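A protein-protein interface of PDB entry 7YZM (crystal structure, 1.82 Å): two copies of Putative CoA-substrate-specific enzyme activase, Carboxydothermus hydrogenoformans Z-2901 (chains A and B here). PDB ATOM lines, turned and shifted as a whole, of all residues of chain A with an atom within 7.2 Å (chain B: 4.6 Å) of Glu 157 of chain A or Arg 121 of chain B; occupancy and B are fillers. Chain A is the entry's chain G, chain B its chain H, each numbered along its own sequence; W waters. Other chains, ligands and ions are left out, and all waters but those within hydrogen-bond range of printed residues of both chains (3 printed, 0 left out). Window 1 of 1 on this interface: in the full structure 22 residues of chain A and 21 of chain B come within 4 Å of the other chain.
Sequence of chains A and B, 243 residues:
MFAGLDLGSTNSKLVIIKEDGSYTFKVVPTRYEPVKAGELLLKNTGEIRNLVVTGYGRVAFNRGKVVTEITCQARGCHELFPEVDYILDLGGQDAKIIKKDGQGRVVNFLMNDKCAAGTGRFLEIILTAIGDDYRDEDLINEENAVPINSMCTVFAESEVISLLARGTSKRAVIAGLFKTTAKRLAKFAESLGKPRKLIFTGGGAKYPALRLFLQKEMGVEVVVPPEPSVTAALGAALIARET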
ATOM      1  N   PHE A 122      18.359  -4.668 -10.001  1.00  0.00           N
ATOM      2  CA  PHE A 122      18.401  -3.421  -9.243  1.00  0.00           C
ATOM      3  C   PHE A 122      17.913  -2.251 -10.089  1.00  0.00           C
ATOM      4  O   PHE A 122      17.153  -1.400  -9.606  1.00  0.00           O
ATOM      5  CB  PHE A 122      19.820  -3.163  -8.728  1.00  0.00           C
ATOM      6  CG  PHE A 122      19.983  -1.832  -8.053  1.00  0.00           C
ATOM      7  CD1 PHE A 122      19.379  -1.580  -6.830  1.00  0.00           C
ATOM      8  CD2 PHE A 122      20.727  -0.824  -8.645  1.00  0.00           C
ATOM      9  CE1 PHE A 122      19.517  -0.344  -6.210  1.00  0.00           C
ATOM     10  CE2 PHE A 122      20.871   0.414  -8.026  1.00  0.00           C
ATOM     11  CZ  PHE A 122      20.268   0.652  -6.810  1.00  0.00           C
ATOM     12  N   ILE A 125      14.121  -2.518 -10.256  1.00  0.00           N
ATOM     13  CA  ILE A 125      13.447  -2.143  -9.018  1.00  0.00           C
ATOM     14  C   ILE A 125      13.481  -0.634  -8.822  1.00  0.00           C
ATOM     15  O   ILE A 125      12.490  -0.023  -8.405  1.00  0.00           O
ATOM     16  CB  ILE A 125      14.100  -2.861  -7.823  1.00  0.00           C
ATOM     17  CG1 ILE A 125      13.774  -4.353  -7.820  1.00  0.00           C
ATOM     18  CG2 ILE A 125      13.651  -2.225  -6.514  1.00  0.00           C
ATOM     19  CD1 ILE A 125      14.654  -5.152  -6.878  1.00  0.00           C
ATOM     20  N   ILE A 126      14.636  -0.019  -9.066  1.00  0.00           N
ATOM     21  CA  ILE A 126      14.796   1.397  -8.789  1.00  0.00           C
ATOM     22  C   ILE A 126      13.989   2.220  -9.782  1.00  0.00           C
ATOM     23  O   ILE A 126      13.386   3.235  -9.419  1.00  0.00           O
ATOM     24  CB  ILE A 126      16.294   1.758  -8.796  1.00  0.00           C
ATOM     25  CG1 ILE A 126      16.630   2.741  -7.677  1.00  0.00           C
ATOM     26  CG2 ILE A 126      16.707   2.328 -10.141  1.00  0.00           C
ATOM     27  CD1 ILE A 126      16.619   2.129  -6.294  1.00  0.00           C
ATOM     28  N   ALA A 129      10.439   2.191  -8.676  1.00  0.00           N
ATOM     29  CA  ALA A 129      10.227   3.027  -7.524  1.00  0.00           C
ATOM     30  C   ALA A 129      10.160   4.522  -7.898  1.00  0.00           C
ATOM     31  O   ALA A 129       9.375   5.309  -7.334  1.00  0.00           O
ATOM     32  CB  ALA A 129      11.251   2.769  -6.388  1.00  0.00           C
ATOM     33  N   ILE A 148      27.462   7.771  -8.908  1.00  0.00           N
ATOM     34  CA  ILE A 148      26.926   6.826  -7.936  1.00  0.00           C
ATOM     35  C   ILE A 148      27.933   5.698  -7.787  1.00  0.00           C
ATOM     36  O   ILE A 148      28.557   5.287  -8.769  1.00  0.00           O
ATOM     37  CB  ILE A 148      25.543   6.293  -8.367  1.00  0.00           C
ATOM     38  CG1 ILE A 148      24.560   7.463  -8.439  1.00  0.00           C
ATOM     39  CG2 ILE A 148      25.048   5.222  -7.399  1.00  0.00           C
ATOM     40  CD1 ILE A 148      23.209   7.109  -8.984  1.00  0.00           C
ATOM     41  N   ASN A 149      28.098   5.199  -6.562  1.00  0.00           N
ATOM     42  CA  ASN A 149      29.125   4.196  -6.317  1.00  0.00           C
ATOM     43  C   ASN A 149      28.967   3.024  -7.279  1.00  0.00           C
ATOM     44  O   ASN A 149      27.857   2.539  -7.521  1.00  0.00           O
ATOM     45  CB  ASN A 149      29.076   3.695  -4.873  1.00  0.00           C
ATOM     46  CG  ASN A 149      30.398   3.085  -4.429  1.00  0.00           C
ATOM     47  OD1 ASN A 149      31.122   2.494  -5.234  1.00  0.00           O
ATOM     48  ND2 ASN A 149      30.733   3.254  -3.153  1.00  0.00           N
ATOM     49  N   CYS A 152      28.599  -2.012  -5.975  1.00  0.00           N
ATOM     50  CA  CYS A 152      27.575  -3.048  -5.900  1.00  0.00           C
ATOM     51  C   CYS A 152      26.240  -2.354  -5.674  1.00  0.00           C
ATOM     52  O   CYS A 152      26.184  -1.149  -5.432  1.00  0.00           O
ATOM     53  CB  CYS A 152      27.859  -4.031  -4.768  1.00  0.00           C
ATOM     54  SG  CYS A 152      27.717  -3.183  -3.193  1.00  0.00           S
ATOM     55  N   THR A 153      25.163  -3.137  -5.748  1.00  0.00           N
ATOM     56  CA  THR A 153      23.833  -2.560  -5.601  1.00  0.00           C
ATOM     57  C   THR A 153      23.528  -2.172  -4.159  1.00  0.00           C
ATOM     58  O   THR A 153      22.692  -1.295  -3.934  1.00  0.00           O
ATOM     59  CB  THR A 153      22.772  -3.534  -6.121  1.00  0.00           C
ATOM     60  OG1 THR A 153      22.851  -4.774  -5.406  1.00  0.00           O
ATOM     61  CG2 THR A 153      22.978  -3.800  -7.610  1.00  0.00           C
ATOM     62  N   VAL A 154      24.183  -2.799  -3.180  1.00  0.00           N
ATOM     63  CA  VAL A 154      24.005  -2.374  -1.794  1.00  0.00           C
ATOM     64  C   VAL A 154      24.504  -0.944  -1.621  1.00  0.00           C
ATOM     65  O   VAL A 154      23.789  -0.077  -1.104  1.00  0.00           O
ATOM     66  CB  VAL A 154      24.722  -3.341  -0.834  1.00  0.00           C
ATOM     67  CG1 VAL A 154      24.750  -2.764   0.581  1.00  0.00           C
ATOM     68  CG2 VAL A 154      24.038  -4.699  -0.852  1.00  0.00           C
ATOM     69  N   PHE A 155      25.743  -0.678  -2.050  1.00  0.00           N
ATOM     70  CA  PHE A 155      26.300   0.662  -1.906  1.00  0.00           C
ATOM     71  C   PHE A 155      25.508   1.669  -2.733  1.00  0.00           C
ATOM     72  O   PHE A 155      25.258   2.793  -2.286  1.00  0.00           O
ATOM     73  CB  PHE A 155      27.778   0.675  -2.317  1.00  0.00           C
ATOM     74  CG  PHE A 155      28.693  -0.096  -1.385  1.00  0.00           C
ATOM     75  CD1 PHE A 155      28.184  -1.003  -0.468  1.00  0.00           C
ATOM     76  CD2 PHE A 155      30.066   0.083  -1.445  1.00  0.00           C
ATOM     77  CE1 PHE A 155      29.029  -1.710   0.374  1.00  0.00           C
ATOM     78  CE2 PHE A 155      30.912  -0.618  -0.604  1.00  0.00           C
ATOM     79  CZ  PHE A 155      30.390  -1.515   0.306  1.00  0.00           C
ATOM     80  N   ALA A 156      25.086   1.279  -3.935  1.00  0.00           N
ATOM     81  CA  ALA A 156      24.345   2.203  -4.787  1.00  0.00           C
ATOM     82  C   ALA A 156      22.985   2.544  -4.187  1.00  0.00           C
ATOM     83  O   ALA A 156      22.562   3.707  -4.216  1.00  0.00           O
ATOM     84  CB  ALA A 156      24.180   1.604  -6.183  1.00  0.00           C
ATOM     85  N   GLU A 157      22.279   1.539  -3.656  1.00  0.00           N
ATOM     86  CA  GLU A 157      21.005   1.794  -2.995  1.00  0.00           C
ATOM     87  C   GLU A 157      21.182   2.758  -1.833  1.00  0.00           C
ATOM     88  O   GLU A 157      20.367   3.664  -1.635  1.00  0.00           O
ATOM     89  CB  GLU A 157      20.392   0.487  -2.491  1.00  0.00           C
ATOM     90  CG  GLU A 157      19.071   0.692  -1.759  1.00  0.00           C
ATOM     91  CD  GLU A 157      18.546  -0.572  -1.115  1.00  0.00           C
ATOM     92  OE1 GLU A 157      19.294  -1.574  -1.070  1.00  0.00           O
ATOM     93  OE2 GLU A 157      17.384  -0.561  -0.654  1.00  0.00           O
ATOM     94  N   SER A 158      22.241   2.563  -1.046  1.00  0.00           N
ATOM     95  CA  SER A 158      22.519   3.477   0.055  1.00  0.00           C
ATOM     96  C   SER A 158      22.661   4.908  -0.450  1.00  0.00           C
ATOM     97  O   SER A 158      22.134   5.844   0.158  1.00  0.00           O
ATOM     98  CB  SER A 158      23.782   3.036   0.796  1.00  0.00           C
ATOM     99  OG  SER A 158      23.548   1.843   1.523  1.00  0.00           O
ATOM    100  N   GLU A 159      23.353   5.096  -1.574  1.00  0.00           N
ATOM    101  CA  GLU A 159      23.581   6.448  -2.072  1.00  0.00           C
ATOM    102  C   GLU A 159      22.318   7.032  -2.684  1.00  0.00           C
ATOM    103  O   GLU A 159      22.033   8.223  -2.517  1.00  0.00           O
ATOM    104  CB  GLU A 159      24.727   6.438  -3.081  1.00  0.00           C
ATOM    105  CG  GLU A 159      26.030   5.931  -2.475  1.00  0.00           C
ATOM    106  CD  GLU A 159      27.249   6.404  -3.229  1.00  0.00           C
ATOM    107  OE1 GLU A 159      27.115   6.685  -4.439  1.00  0.00           O
ATOM    108  OE2 GLU A 159      28.334   6.500  -2.612  1.00  0.00           O
ATOM    109  N   VAL A 160      21.545   6.204  -3.387  1.00  0.00           N
ATOM    110  CA  VAL A 160      20.264   6.654  -3.921  1.00  0.00           C
ATOM    111  C   VAL A 160      19.368   7.159  -2.795  1.00  0.00           C
ATOM    112  O   VAL A 160      18.698   8.189  -2.930  1.00  0.00           O
ATOM    113  CB  VAL A 160      19.595   5.518  -4.712  1.00  0.00           C
ATOM    114  CG1 VAL A 160      18.142   5.843  -4.990  1.00  0.00           C
ATOM    115  CG2 VAL A 160      20.350   5.274  -6.006  1.00  0.00           C
ATOM    116  N   ILE A 161      19.335   6.442  -1.674  1.00  0.00           N
ATOM    117  CA  ILE A 161      18.507   6.875  -0.552  1.00  0.00           C
ATOM    118  C   ILE A 161      18.953   8.250  -0.073  1.00  0.00           C
ATOM    119  O   ILE A 161      18.136   9.162   0.100  1.00  0.00           O
ATOM    120  CB  ILE A 161      18.552   5.836   0.584  1.00  0.00           C
ATOM    121  CG1 ILE A 161      17.627   4.659   0.258  1.00  0.00           C
ATOM    122  CG2 ILE A 161      18.139   6.466   1.906  1.00  0.00           C
ATOM    123  CD1 ILE A 161      17.917   3.406   1.060  1.00  0.00           C
ATOM    124  N   SER A 162      20.262   8.415   0.160  1.00  0.00           N
ATOM    125  CA  SER A 162      20.778   9.698   0.632  1.00  0.00           C
ATOM    126  C   SER A 162      20.531  10.804  -0.387  1.00  0.00           C
ATOM    127  O   SER A 162      20.208  11.941  -0.020  1.00  0.00           O
ATOM    128  CB  SER A 162      22.276   9.589   0.926  1.00  0.00           C
ATOM    129  OG  SER A 162      22.527   8.760   2.045  1.00  0.00           O
ATOM    130  N   LEU A 163      20.678  10.488  -1.674  1.00  0.00           N
ATOM    131  CA  LEU A 163      20.539  11.508  -2.707  1.00  0.00           C
ATOM    132  C   LEU A 163      19.111  12.033  -2.777  1.00  0.00           C
ATOM    133  O   LEU A 163      18.889  13.247  -2.843  1.00  0.00           O
ATOM    134  CB  LEU A 163      20.969  10.938  -4.057  1.00  0.00           C
ATOM    135  CG  LEU A 163      22.471  10.925  -4.342  1.00  0.00           C
ATOM    136  CD1 LEU A 163      22.755  10.135  -5.619  1.00  0.00           C
ATOM    137  CD2 LEU A 163      23.004  12.342  -4.442  1.00  0.00           C
ATOM    138  N   LEU A 177      22.598   6.720 -12.389  1.00  0.00           N
ATOM    139  CA  LEU A 177      22.611   5.262 -12.326  1.00  0.00           C
ATOM    140  C   LEU A 177      22.978   4.667 -13.678  1.00  0.00           C
ATOM    141  O   LEU A 177      23.834   3.781 -13.768  1.00  0.00           O
ATOM    142  CB  LEU A 177      21.249   4.740 -11.869  1.00  0.00           C
ATOM    143  CG  LEU A 177      20.953   4.816 -10.369  1.00  0.00           C
ATOM    144  CD1 LEU A 177      19.476   4.524 -10.114  1.00  0.00           C
ATOM    145  CD2 LEU A 177      21.825   3.865  -9.572  1.00  0.00           C
ATOM    146  N   GLY B  92      14.496  -0.256   7.251  1.00  0.00           N
ATOM    147  CA  GLY B  92      14.617  -0.691   5.869  1.00  0.00           C
ATOM    148  C   GLY B  92      16.015  -0.585   5.300  1.00  0.00           C
ATOM    149  O   GLY B  92      16.381  -1.358   4.407  1.00  0.00           O
ATOM    150  N   GLN B  93      16.801   0.363   5.786  1.00  0.00           N
ATOM    151  CA  GLN B  93      18.164   0.571   5.318  1.00  0.00           C
ATOM    152  C   GLN B  93      19.207   0.326   6.395  1.00  0.00           C
ATOM    153  O   GLN B  93      20.251  -0.267   6.103  1.00  0.00           O
ATOM    154  CB  GLN B  93      18.314   1.995   4.759  1.00  0.00           C
ATOM    155  CG  GLN B  93      19.750   2.521   4.646  1.00  0.00           C
ATOM    156  CD  GLN B  93      20.588   1.863   3.552  1.00  0.00           C
ATOM    157  OE1 GLN B  93      21.795   2.100   3.469  1.00  0.00           O
ATOM    158  NE2 GLN B  93      19.959   1.046   2.713  1.00  0.00           N
ATOM    159  N   GLY B 118      20.564  -2.238   4.047  1.00  0.00           N
ATOM    160  CA  GLY B 118      19.422  -2.594   3.228  1.00  0.00           C
ATOM    161  C   GLY B 118      18.767  -3.922   3.518  1.00  0.00           C
ATOM    162  O   GLY B 118      17.990  -4.397   2.688  1.00  0.00           O
ATOM    163  N   THR B 119      19.033  -4.533   4.674  1.00  0.00           N
ATOM    164  CA  THR B 119      18.467  -5.846   4.968  1.00  0.00           C
ATOM    165  C   THR B 119      16.941  -5.807   4.985  1.00  0.00           C
ATOM    166  O   THR B 119      16.278  -6.683   4.412  1.00  0.00           O
ATOM    167  CB  THR B 119      18.996  -6.360   6.309  1.00  0.00           C
ATOM    168  OG1 THR B 119      20.418  -6.502   6.241  1.00  0.00           O
ATOM    169  CG2 THR B 119      18.389  -7.708   6.647  1.00  0.00           C
ATOM    170  N   GLY B 120      16.363  -4.805   5.653  1.00  0.00           N
ATOM    171  CA  GLY B 120      14.912  -4.759   5.778  1.00  0.00           C
ATOM    172  C   GLY B 120      14.210  -4.622   4.440  1.00  0.00           C
ATOM    173  O   GLY B 120      13.232  -5.318   4.162  1.00  0.00           O
ATOM    174  N   ARG B 121      14.696  -3.708   3.601  1.00  0.00           N
ATOM    175  CA  ARG B 121      14.108  -3.518   2.279  1.00  0.00           C
ATOM    176  C   ARG B 121      14.263  -4.774   1.427  1.00  0.00           C
ATOM    177  O   ARG B 121      13.366  -5.121   0.652  1.00  0.00           O
ATOM    178  CB  ARG B 121      14.752  -2.298   1.619  1.00  0.00           C
ATOM    179  CG  ARG B 121      14.416  -2.102   0.167  1.00  0.00           C
ATOM    180  CD  ARG B 121      13.022  -1.526  -0.021  1.00  0.00           C
ATOM    181  NE  ARG B 121      12.801  -1.210  -1.431  1.00  0.00           N
ATOM    182  CZ  ARG B 121      11.678  -1.458  -2.100  1.00  0.00           C
ATOM    183  NH1 ARG B 121      10.640  -2.023  -1.495  1.00  0.00           N
ATOM    184  NH2 ARG B 121      11.596  -1.135  -3.386  1.00  0.00           N
ATOM    185  N   PHE B 122      15.386  -5.479   1.562  1.00  0.00           N
ATOM    186  CA  PHE B 122      15.540  -6.729   0.827  1.00  0.00           C
ATOM    187  C   PHE B 122      14.498  -7.750   1.259  1.00  0.00           C
ATOM    188  O   PHE B 122      13.896  -8.430   0.422  1.00  0.00           O
ATOM    189  CB  PHE B 122      16.943  -7.282   1.040  1.00  0.00           C
ATOM    190  CG  PHE B 122      17.118  -8.698   0.585  1.00  0.00           C
ATOM    191  CD1 PHE B 122      17.227  -8.999  -0.759  1.00  0.00           C
ATOM    192  CD2 PHE B 122      17.188  -9.725   1.503  1.00  0.00           C
ATOM    193  CE1 PHE B 122      17.404 -10.311  -1.176  1.00  0.00           C
ATOM    194  CE2 PHE B 122      17.366 -11.030   1.095  1.00  0.00           C
ATOM    195  CZ  PHE B 122      17.477 -11.322  -0.244  1.00  0.00           C
ATOM    196  N   LEU B 123      14.283  -7.885   2.568  1.00  0.00           N
ATOM    197  CA  LEU B 123      13.272  -8.819   3.043  1.00  0.00           C
ATOM    198  C   LEU B 123      11.902  -8.449   2.496  1.00  0.00           C
ATOM    199  O   LEU B 123      11.143  -9.323   2.069  1.00  0.00           O
ATOM    200  CB  LEU B 123      13.253  -8.847   4.568  1.00  0.00           C
ATOM    201  CG  LEU B 123      14.490  -9.470   5.214  1.00  0.00           C
ATOM    202  CD1 LEU B 123      14.430  -9.267   6.713  1.00  0.00           C
ATOM    203  CD2 LEU B 123      14.610 -10.941   4.872  1.00  0.00           C
ATOM    204  N   GLU B 124      11.572  -7.156   2.498  1.00  0.00           N
ATOM    205  CA  GLU B 124      10.304  -6.719   1.928  1.00  0.00           C
ATOM    206  C   GLU B 124      10.223  -7.096   0.455  1.00  0.00           C
ATOM    207  O   GLU B 124       9.212  -7.632  -0.003  1.00  0.00           O
ATOM    208  CB  GLU B 124      10.125  -5.209   2.107  1.00  0.00           C
ATOM    209  CG  GLU B 124       8.725  -4.716   1.742  1.00  0.00           C
ATOM    210  CD  GLU B 124       8.629  -3.201   1.559  1.00  0.00           C
ATOM    211  OE1 GLU B 124       9.667  -2.506   1.615  1.00  0.00           O
ATOM    212  OE2 GLU B 124       7.500  -2.709   1.350  1.00  0.00           O
ATOM    213  N   ILE B 125      11.294  -6.840  -0.298  1.00  0.00           N
ATOM    214  CA  ILE B 125      11.292  -7.117  -1.732  1.00  0.00           C
ATOM    215  C   ILE B 125      11.107  -8.607  -1.983  1.00  0.00           C
ATOM    216  O   ILE B 125      10.267  -9.027  -2.791  1.00  0.00           O
ATOM    217  CB  ILE B 125      12.599  -6.610  -2.372  1.00  0.00           C
ATOM    218  CG1 ILE B 125      12.633  -5.081  -2.424  1.00  0.00           C
ATOM    219  CG2 ILE B 125      12.773  -7.184  -3.772  1.00  0.00           C
ATOM    220  CD1 ILE B 125      14.035  -4.511  -2.643  1.00  0.00           C
HETATM  221  O   HOH W   1      21.572  -0.608   0.805  1.00  0.00           O
HETATM  222  O   HOH W   2      17.212   0.204   2.047  1.00  0.00           O
HETATM  223  O   HOH W   3      17.943  -3.794   0.105  1.00  0.00           O
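The side-chain hydroxyl (OG) of Ser 158 of chain A lies within hydrogen-bond range of the side-chain amide oxygen (OE1) of Gln 93 of chain B.
OG of Ser 158 of chain A lies within hydrogen-bond range of O of Val 154 of chain A (3.3 Å). The side-chain hydroxyl of Ser 162 of chain A is in hydrogen-bond range of the backbone carbonyl oxygen of Ser 158 of chain A (3.5 Å). The backbone NH of Arg 121 of chain B is in hydrogen-bond range of the backbone carbonyl oxygen of Gly 92 of chain B. The guanidinium group (NH1) of Arg 121 of chain B is in salt-bridge range of the side-chain carboxylate (OE1) of Glu 124 of chain B (3.3 Å). The backbone carbonyl oxygen (O) of Gln 93 of chain B is in hydrogen-bond range of the backbone NH (N) of Gly 118 of chain B, 2.9 Å away.
CG2 of Ile 125 of chain A touches NH2 of Arg 121 of chain B, at 3.9 Å. Glu 157 of chain A touches Arg 121 of chain B. NE2 of Gln 93 of chain B touches CD1 of Ile 161 of chain A, 3.5 Å away.
Arg 121 of chain B touches just these residues of chain A: Ile 125 and Glu 157. Printed residues of chain B within 4 Å of Ile 161 of chain A: Gln 93. Of the printed residues of chain A, Gln 93 of chain B touches Ser 158 (2.6 Å) and Ile 161 (3.5 Å). Of the printed residues of chain B, Ile 125 of chain A touches Arg 121. Printed residues of chain B within 4 Å of Ser 158 of chain A: Gln 93 (2.6 Å). Gly 92 of chain B touches none of the printed residues of chain A. Ala 156 of chain A touches none of the printed residues of chain B. The nearest residue of chain A that does not touch Arg 121 of chain B is Ala 129 of chain A (4.9 Å). The nearest printed residue of chain A that does not touch Gln 93 of chain B is Glu 157 of chain A (4.4 Å).
Among the printed residues, 4 pairs touch across the chains.
2 positions are printed for both chains. Of the 4 pairs that touch across the chains among the printed residues, none has its exchanged pair printed and touching as well.
Water W3 lies within hydrogen-bond range of the backbone carbonyl oxygen (O) of Gly 118 of chain B (2.7 Å), the side-chain carboxylate (OE1) of Glu 157 of chain A (2.9 Å) and the backbone NH (N) of Phe 122 of chain B (3.4 Å). Water W2 lies within hydrogen-bond range of OE2 of Glu 157 of chain A (2.8 Å), O of Gly 92 of chain B (2.9 Å) and NE2 of Gln 93 of chain B (2.9 Å). Water W1 lies within hydrogen-bond range of the backbone carbonyl oxygen of Val 154 of chain A (3.0 Å), the side-chain amide nitrogen of Gln 93 of chain B (3.0 Å), the side-chain carboxylate of Glu 157 of chain A (3.1 Å) and the side-chain hydroxyl of Ser 158 of chain A (3.2 Å).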
